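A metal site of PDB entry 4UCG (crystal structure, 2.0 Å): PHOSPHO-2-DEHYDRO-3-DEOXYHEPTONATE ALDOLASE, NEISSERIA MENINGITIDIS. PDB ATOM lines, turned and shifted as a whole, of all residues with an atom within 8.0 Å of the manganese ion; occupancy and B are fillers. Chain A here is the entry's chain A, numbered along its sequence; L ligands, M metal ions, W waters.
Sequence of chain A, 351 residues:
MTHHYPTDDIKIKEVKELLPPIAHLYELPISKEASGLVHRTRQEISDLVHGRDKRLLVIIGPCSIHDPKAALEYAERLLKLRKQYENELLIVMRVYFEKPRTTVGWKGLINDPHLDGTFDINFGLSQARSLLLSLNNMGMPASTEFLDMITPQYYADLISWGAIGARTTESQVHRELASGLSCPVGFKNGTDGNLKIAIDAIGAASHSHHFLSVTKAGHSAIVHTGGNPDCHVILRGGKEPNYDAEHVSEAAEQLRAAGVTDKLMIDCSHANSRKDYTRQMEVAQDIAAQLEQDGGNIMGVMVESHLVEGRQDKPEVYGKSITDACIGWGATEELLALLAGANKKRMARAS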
ATOM      1  N   GLY A  61       7.442   0.950 -15.103  1.00  0.00           N
ATOM      2  CA  GLY A  61       8.045   2.242 -14.839  1.00  0.00           C
ATOM      3  C   GLY A  61       9.440   2.282 -15.431  1.00  0.00           C
ATOM      4  O   GLY A  61       9.828   1.432 -16.250  1.00  0.00           O
ATOM      5  N   PRO A  62      10.200   3.316 -15.063  1.00  0.00           N
ATOM      6  CA  PRO A  62      11.473   3.607 -15.707  1.00  0.00           C
ATOM      7  C   PRO A  62      12.467   2.467 -15.644  1.00  0.00           C
ATOM      8  O   PRO A  62      12.453   1.684 -14.712  1.00  0.00           O
ATOM      9  CB  PRO A  62      11.983   4.807 -14.919  1.00  0.00           C
ATOM     10  CG  PRO A  62      10.715   5.514 -14.509  1.00  0.00           C
ATOM     11  CD  PRO A  62       9.784   4.401 -14.144  1.00  0.00           C
ATOM     12  N   CYS A  63      13.339   2.364 -16.630  1.00  0.00           N
ATOM     13  CA  CYS A  63      14.489   1.454 -16.507  1.00  0.00           C
ATOM     14  C   CYS A  63      15.291   1.774 -15.240  1.00  0.00           C
ATOM     15  O   CYS A  63      15.608   0.882 -14.432  1.00  0.00           O
ATOM     16  CB  CYS A  63      15.368   1.523 -17.752  1.00  0.00           C
ATOM     17  SG  CYS A  63      16.884   0.547 -17.638  1.00  0.00           S
ATOM     18  N   SER A  64      15.551   3.070 -15.030  1.00  0.00           N
ATOM     19  CA  SER A  64      16.273   3.548 -13.864  1.00  0.00           C
ATOM     20  C   SER A  64      15.672   4.833 -13.398  1.00  0.00           C
ATOM     21  O   SER A  64      15.131   5.600 -14.209  1.00  0.00           O
ATOM     22  CB  SER A  64      17.739   3.840 -14.216  1.00  0.00           C
ATOM     23  OG  SER A  64      17.843   4.751 -15.306  1.00  0.00           O
ATOM     24  N   ARG A  94       8.194   0.481 -11.057  1.00  0.00           N
ATOM     25  CA  ARG A  94       9.638   0.216 -11.100  1.00  0.00           C
ATOM     26  C   ARG A  94      10.367   1.420 -10.538  1.00  0.00           C
ATOM     27  O   ARG A  94      10.236   2.523 -11.077  1.00  0.00           O
ATOM     28  CB  ARG A  94      10.141  -0.014 -12.548  1.00  0.00           C
ATOM     29  CG  ARG A  94       9.867  -1.371 -13.132  1.00  0.00           C
ATOM     30  CD  ARG A  94      10.320  -1.476 -14.594  1.00  0.00           C
ATOM     31  NE  ARG A  94      11.725  -1.146 -14.699  1.00  0.00           N
ATOM     32  CZ  ARG A  94      12.705  -2.025 -14.825  1.00  0.00           C
ATOM     33  NH1 ARG A  94      12.464  -3.317 -14.992  1.00  0.00           N
ATOM     34  NH2 ARG A  94      13.952  -1.601 -14.828  1.00  0.00           N
ATOM     35  N   TYR A  96      13.974   1.599  -9.739  1.00  0.00           N
ATOM     36  CA  TYR A  96      15.266   0.937  -9.769  1.00  0.00           C
ATOM     37  C   TYR A  96      16.416   1.916  -9.510  1.00  0.00           C
ATOM     38  O   TYR A  96      16.568   2.889 -10.242  1.00  0.00           O
ATOM     39  CB  TYR A  96      15.456   0.253 -11.133  1.00  0.00           C
ATOM     40  CG  TYR A  96      14.750  -1.086 -11.266  1.00  0.00           C
ATOM     41  CD1 TYR A  96      13.436  -1.276 -10.799  1.00  0.00           C
ATOM     42  CD2 TYR A  96      15.389  -2.161 -11.855  1.00  0.00           C
ATOM     43  CE1 TYR A  96      12.792  -2.503 -10.965  1.00  0.00           C
ATOM     44  CE2 TYR A  96      14.773  -3.386 -11.996  1.00  0.00           C
ATOM     45  CZ  TYR A  96      13.492  -3.561 -11.570  1.00  0.00           C
ATOM     46  OH  TYR A  96      12.897  -4.790 -11.722  1.00  0.00           O
ATOM     47  N   LYS A  99      21.854  -0.417 -11.154  1.00  0.00           N
ATOM     48  CA  LYS A  99      21.894  -0.866 -12.538  1.00  0.00           C
ATOM     49  C   LYS A  99      23.153  -1.686 -12.818  1.00  0.00           C
ATOM     50  O   LYS A  99      24.280  -1.220 -12.628  1.00  0.00           O
ATOM     51  CB  LYS A  99      21.817   0.315 -13.485  1.00  0.00           C
ATOM     52  CG  LYS A  99      20.620   1.210 -13.236  1.00  0.00           C
ATOM     53  CD  LYS A  99      19.295   0.456 -13.289  1.00  0.00           C
ATOM     54  CE  LYS A  99      19.120  -0.242 -14.627  1.00  0.00           C
ATOM     55  NZ  LYS A  99      17.795  -0.917 -14.698  1.00  0.00           N
ATOM     56  N   PRO A 100      22.959  -2.914 -13.294  1.00  0.00           N
ATOM     57  CA  PRO A 100      24.095  -3.749 -13.637  1.00  0.00           C
ATOM     58  C   PRO A 100      24.540  -3.458 -15.059  1.00  0.00           C
ATOM     59  O   PRO A 100      23.764  -3.633 -15.976  1.00  0.00           O
ATOM     60  CB  PRO A 100      23.529  -5.156 -13.510  1.00  0.00           C
ATOM     61  CG  PRO A 100      22.079  -5.018 -13.832  1.00  0.00           C
ATOM     62  CD  PRO A 100      21.674  -3.611 -13.478  1.00  0.00           C
ATOM     63  N   GLU A 145      15.554  -3.723  -8.400  1.00  0.00           N
ATOM     64  CA  GLU A 145      16.532  -4.817  -8.474  1.00  0.00           C
ATOM     65  C   GLU A 145      17.507  -4.671  -7.316  1.00  0.00           C
ATOM     66  O   GLU A 145      18.153  -3.638  -7.143  1.00  0.00           O
ATOM     67  CB  GLU A 145      17.349  -4.830  -9.767  1.00  0.00           C
ATOM     68  CG  GLU A 145      18.501  -5.877  -9.710  1.00  0.00           C
ATOM     69  CD  GLU A 145      19.350  -5.996 -10.977  1.00  0.00           C
ATOM     70  OE1 GLU A 145      18.973  -5.473 -12.088  1.00  0.00           O
ATOM     71  OE2 GLU A 145      20.428  -6.649 -10.846  1.00  0.00           O
ATOM     72  N   ARG A 167      22.012 -11.153 -14.716  1.00  0.00           N
ATOM     73  CA  ARG A 167      23.454 -11.289 -14.591  1.00  0.00           C
ATOM     74  C   ARG A 167      23.916 -11.756 -13.226  1.00  0.00           C
ATOM     75  O   ARG A 167      25.098 -11.982 -13.023  1.00  0.00           O
ATOM     76  CB  ARG A 167      24.122  -9.928 -14.865  1.00  0.00           C
ATOM     77  CG  ARG A 167      23.930  -9.458 -16.293  1.00  0.00           C
ATOM     78  CD  ARG A 167      24.385  -8.017 -16.447  1.00  0.00           C
ATOM     79  NE  ARG A 167      24.031  -7.562 -17.789  1.00  0.00           N
ATOM     80  CZ  ARG A 167      22.797  -7.247 -18.184  1.00  0.00           C
ATOM     81  NH1 ARG A 167      21.757  -7.243 -17.344  1.00  0.00           N
ATOM     82  NH2 ARG A 167      22.619  -6.888 -19.449  1.00  0.00           N
ATOM     83  N   LYS A 188      15.474 -13.473 -12.750  1.00  0.00           N
ATOM     84  CA  LYS A 188      15.456 -13.466 -14.205  1.00  0.00           C
ATOM     85  C   LYS A 188      16.269 -14.637 -14.742  1.00  0.00           C
ATOM     86  O   LYS A 188      17.293 -15.015 -14.156  1.00  0.00           O
ATOM     87  CB  LYS A 188      16.005 -12.126 -14.720  1.00  0.00           C
ATOM     88  CG  LYS A 188      15.037 -10.969 -14.477  1.00  0.00           C
ATOM     89  CD  LYS A 188      15.386  -9.708 -15.223  1.00  0.00           C
ATOM     90  CE  LYS A 188      14.123  -8.956 -15.627  1.00  0.00           C
ATOM     91  NZ  LYS A 188      14.474  -7.788 -16.454  1.00  0.00           N
ATOM     92  N   ASP A 267       8.857 -10.484 -18.732  1.00  0.00           N
ATOM     93  CA  ASP A 267       9.371  -9.139 -19.027  1.00  0.00           C
ATOM     94  C   ASP A 267       9.102  -8.842 -20.492  1.00  0.00           C
ATOM     95  O   ASP A 267       9.530  -9.599 -21.354  1.00  0.00           O
ATOM     96  CB  ASP A 267      10.882  -9.087 -18.725  1.00  0.00           C
ATOM     97  CG  ASP A 267      11.489  -7.686 -18.842  1.00  0.00           C
ATOM     98  OD1 ASP A 267      10.775  -6.732 -19.173  1.00  0.00           O
ATOM     99  OD2 ASP A 267      12.715  -7.554 -18.615  1.00  0.00           O
ATOM    100  N   SER A 269      10.295  -6.243 -21.927  1.00  0.00           N
ATOM    101  CA  SER A 269      11.463  -5.459 -22.330  1.00  0.00           C
ATOM    102  C   SER A 269      12.743  -6.291 -22.486  1.00  0.00           C
ATOM    103  O   SER A 269      12.692  -7.503 -22.618  1.00  0.00           O
ATOM    104  CB  SER A 269      11.694  -4.289 -21.378  1.00  0.00           C
ATOM    105  OG  SER A 269      12.333  -3.224 -22.035  1.00  0.00           O
ATOM    106  N   HIS A 270      13.884  -5.598 -22.489  1.00  0.00           N
ATOM    107  CA  HIS A 270      15.170  -6.251 -22.612  1.00  0.00           C
ATOM    108  C   HIS A 270      15.213  -7.254 -23.776  1.00  0.00           C
ATOM    109  O   HIS A 270      14.864  -6.894 -24.904  1.00  0.00           O
ATOM    110  CB  HIS A 270      15.581  -6.838 -21.252  1.00  0.00           C
ATOM    111  CG  HIS A 270      15.487  -5.826 -20.171  1.00  0.00           C
ATOM    112  ND1 HIS A 270      14.409  -5.743 -19.324  1.00  0.00           N
ATOM    113  CD2 HIS A 270      16.259  -4.744 -19.914  1.00  0.00           C
ATOM    114  CE1 HIS A 270      14.550  -4.686 -18.545  1.00  0.00           C
ATOM    115  NE2 HIS A 270      15.673  -4.081 -18.865  1.00  0.00           N
ATOM    116  N   MET A 302       6.371  -7.366 -16.774  1.00  0.00           N
ATOM    117  CA  MET A 302       7.281  -6.265 -16.526  1.00  0.00           C
ATOM    118  C   MET A 302       7.380  -5.396 -17.772  1.00  0.00           C
ATOM    119  O   MET A 302       7.389  -5.911 -18.907  1.00  0.00           O
ATOM    120  CB  MET A 302       8.653  -6.813 -16.118  1.00  0.00           C
ATOM    121  CG  MET A 302       9.686  -5.763 -15.723  1.00  0.00           C
ATOM    122  SD  MET A 302      11.292  -6.526 -15.219  1.00  0.00           S
ATOM    123  CE  MET A 302      10.707  -7.761 -14.112  1.00  0.00           C
ATOM    124  N   GLU A 304       9.028  -1.484 -19.281  1.00  0.00           N
ATOM    125  CA  GLU A 304       9.877  -0.329 -19.082  1.00  0.00           C
ATOM    126  C   GLU A 304       9.199   0.886 -19.744  1.00  0.00           C
ATOM    127  O   GLU A 304       9.085   0.931 -20.960  1.00  0.00           O
ATOM    128  CB  GLU A 304      11.255  -0.617 -19.665  1.00  0.00           C
ATOM    129  CG  GLU A 304      12.059  -1.553 -18.781  1.00  0.00           C
ATOM    130  CD  GLU A 304      13.534  -1.579 -19.134  1.00  0.00           C
ATOM    131  OE1 GLU A 304      13.851  -1.762 -20.309  1.00  0.00           O
ATOM    132  OE2 GLU A 304      14.378  -1.460 -18.212  1.00  0.00           O
ATOM    133  N   SER A 321      14.378   8.373 -20.245  1.00  0.00           N
ATOM    134  CA  SER A 321      15.365   7.462 -19.665  1.00  0.00           C
ATOM    135  C   SER A 321      16.788   7.834 -20.092  1.00  0.00           C
ATOM    136  O   SER A 321      17.015   8.198 -21.216  1.00  0.00           O
ATOM    137  CB  SER A 321      15.116   6.035 -20.151  1.00  0.00           C
ATOM    138  OG  SER A 321      15.993   5.130 -19.515  1.00  0.00           O
ATOM    139  N   THR A 323      18.981   5.313 -19.274  1.00  0.00           N
ATOM    140  CA  THR A 323      19.418   3.913 -19.442  1.00  0.00           C
ATOM    141  C   THR A 323      18.642   3.273 -20.621  1.00  0.00           C
ATOM    142  O   THR A 323      18.637   3.851 -21.726  1.00  0.00           O
ATOM    143  CB  THR A 323      19.393   3.124 -18.108  1.00  0.00           C
ATOM    144  OG1 THR A 323      18.130   3.269 -17.441  1.00  0.00           O
ATOM    145  CG2 THR A 323      20.480   3.667 -17.210  1.00  0.00           C
ATOM    146  N   ASP A 324      17.980   2.141 -20.433  1.00  0.00           N
ATOM    147  CA  ASP A 324      17.280   1.529 -21.564  1.00  0.00           C
ATOM    148  C   ASP A 324      16.127   2.412 -22.025  1.00  0.00           C
ATOM    149  O   ASP A 324      15.454   3.061 -21.212  1.00  0.00           O
ATOM    150  CB  ASP A 324      16.724   0.140 -21.219  1.00  0.00           C
ATOM    151  CG  ASP A 324      17.804  -0.858 -20.842  1.00  0.00           C
ATOM    152  OD1 ASP A 324      18.928  -0.749 -21.377  1.00  0.00           O
ATOM    153  OD2 ASP A 324      17.528  -1.731 -19.981  1.00  0.00           O
ATOM    154  N   ALA A 325      15.842   2.358 -23.319  1.00  0.00           N
ATOM    155  CA  ALA A 325      14.717   3.107 -23.878  1.00  0.00           C
ATOM    156  C   ALA A 325      13.392   2.567 -23.340  1.00  0.00           C
ATOM    157  O   ALA A 325      13.210   1.363 -23.225  1.00  0.00           O
ATOM    158  CB  ALA A 325      14.748   2.998 -25.388  1.00  0.00           C
ATOM    159  N   CYS A 326      12.464   3.457 -23.019  1.00  0.00           N
ATOM    160  CA  CYS A 326      11.174   3.105 -22.469  1.00  0.00           C
ATOM    161  C   CYS A 326      10.059   3.522 -23.433  1.00  0.00           C
ATOM    162  O   CYS A 326      10.252   4.424 -24.250  1.00  0.00           O
ATOM    163  CB  CYS A 326      10.963   3.828 -21.129  1.00  0.00           C
ATOM    164  SG  CYS A 326      12.147   3.304 -19.860  1.00  0.00           S
HETATM  165  C1  LIG L   1      16.028  -4.326 -15.656  1.00  0.00           C
HETATM  166  O1  LIG L   1      16.093  -3.095 -15.834  1.00  0.00           O
HETATM  167  O2  LIG L   1      14.952  -4.875 -15.271  1.00  0.00           O
HETATM  168  C2  LIG L   1      17.222  -5.171 -15.900  1.00  0.00           C
HETATM  169  C3  LIG L   1      18.452  -4.825 -15.577  1.00  0.00           C
HETATM  170  O3  LIG L   1      16.908  -6.442 -16.547  1.00  0.00           O
HETATM  171  P1  LIG L   1      17.901  -7.624 -17.012  1.00  0.00           P
HETATM  172  O4  LIG L   1      18.434  -8.097 -15.677  1.00  0.00           O
HETATM  173  O5  LIG L   1      16.972  -8.375 -17.899  1.00  0.00           O
HETATM  174  O6  LIG L   1      18.998  -6.899 -17.820  1.00  0.00           O
HETATM  175 MN    MN M   1      16.393  -1.877 -18.329  1.00  0.00          MN
HETATM  176  O   HOH W   1      18.051  -2.177 -17.095  1.00  0.00           O
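The side-chain amino group (NZ) of Lys 99 is in salt-bridge range of an oxygen (O1) of the ligand. The guanidinium group (NH1) of Arg 167 lies within salt-bridge range of an oxygen (O6) of the ligand. The guanidinium group of Arg 94 is in salt-bridge range of an oxygen (O1) of the ligand, 2.8 Å away. A ring nitrogen (NE2) of His 270 sits close to an oxygen (O1) of the ligand, 3.2 Å away. An oxygen (O5) of the ligand is in salt-bridge range of the side-chain amino group (NZ) of Lys 188, at 2.9 Å.
The side-chain sulfur (SG) of Cys 326 sits at hydrogen-bond distance from the backbone carbonyl oxygen (O) of Asp 324 (3.6 Å). The side-chain hydroxyl (OG) of Ser 321 is in hydrogen-bond range of the backbone carbonyl oxygen (O) of Asp 324 (2.7 Å). NZ of Lys 99 lies within hydrogen-bond range of O of Cys 63 (2.8 Å). The side-chain sulfur (SG) of Cys 63 lies close to the side-chain hydroxyl (OG1) of Thr 323, at 3.0 Å. The backbone carbonyl oxygen of Cys 63 lies within hydrogen-bond range of the guanidinium group of Arg 94 (3.0 Å). A ring nitrogen (ND1) of His 270 is in hydrogen-bond range of the side-chain carboxylate (OD2) of Asp 267. The backbone NH (N) of Cys 63 is in hydrogen-bond range of the side-chain sulfur (SG) of Cys 326, at 3.6 Å. The side-chain hydroxyl of Ser 269 is in hydrogen-bond range of the side-chain carboxylate of Glu 304 (2.7 Å).
Of the 21 residues printed, 4 come within 4 Å of the manganese ion. The nearest printed residue that does not touch the manganese ion is Lys 99 (4.01 Å).
The manganese ion is bound by OD2 of Asp 324 (2.0 Å), OE2 of Glu 304 (2.1 Å), water W1 (2.1 Å), NE2 of His 270 (2.4 Å) and SG of Cys 63 (2.6 Å). The manganese ion has five donor atoms within binding distance. Slightly farther from the manganese ion lies an oxygen (O1) of the ligand (2.8 Å).
Water W1 bridges O1 of the ligand (2.5 Å) and NZ of Lys 99 (2.7 Å).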
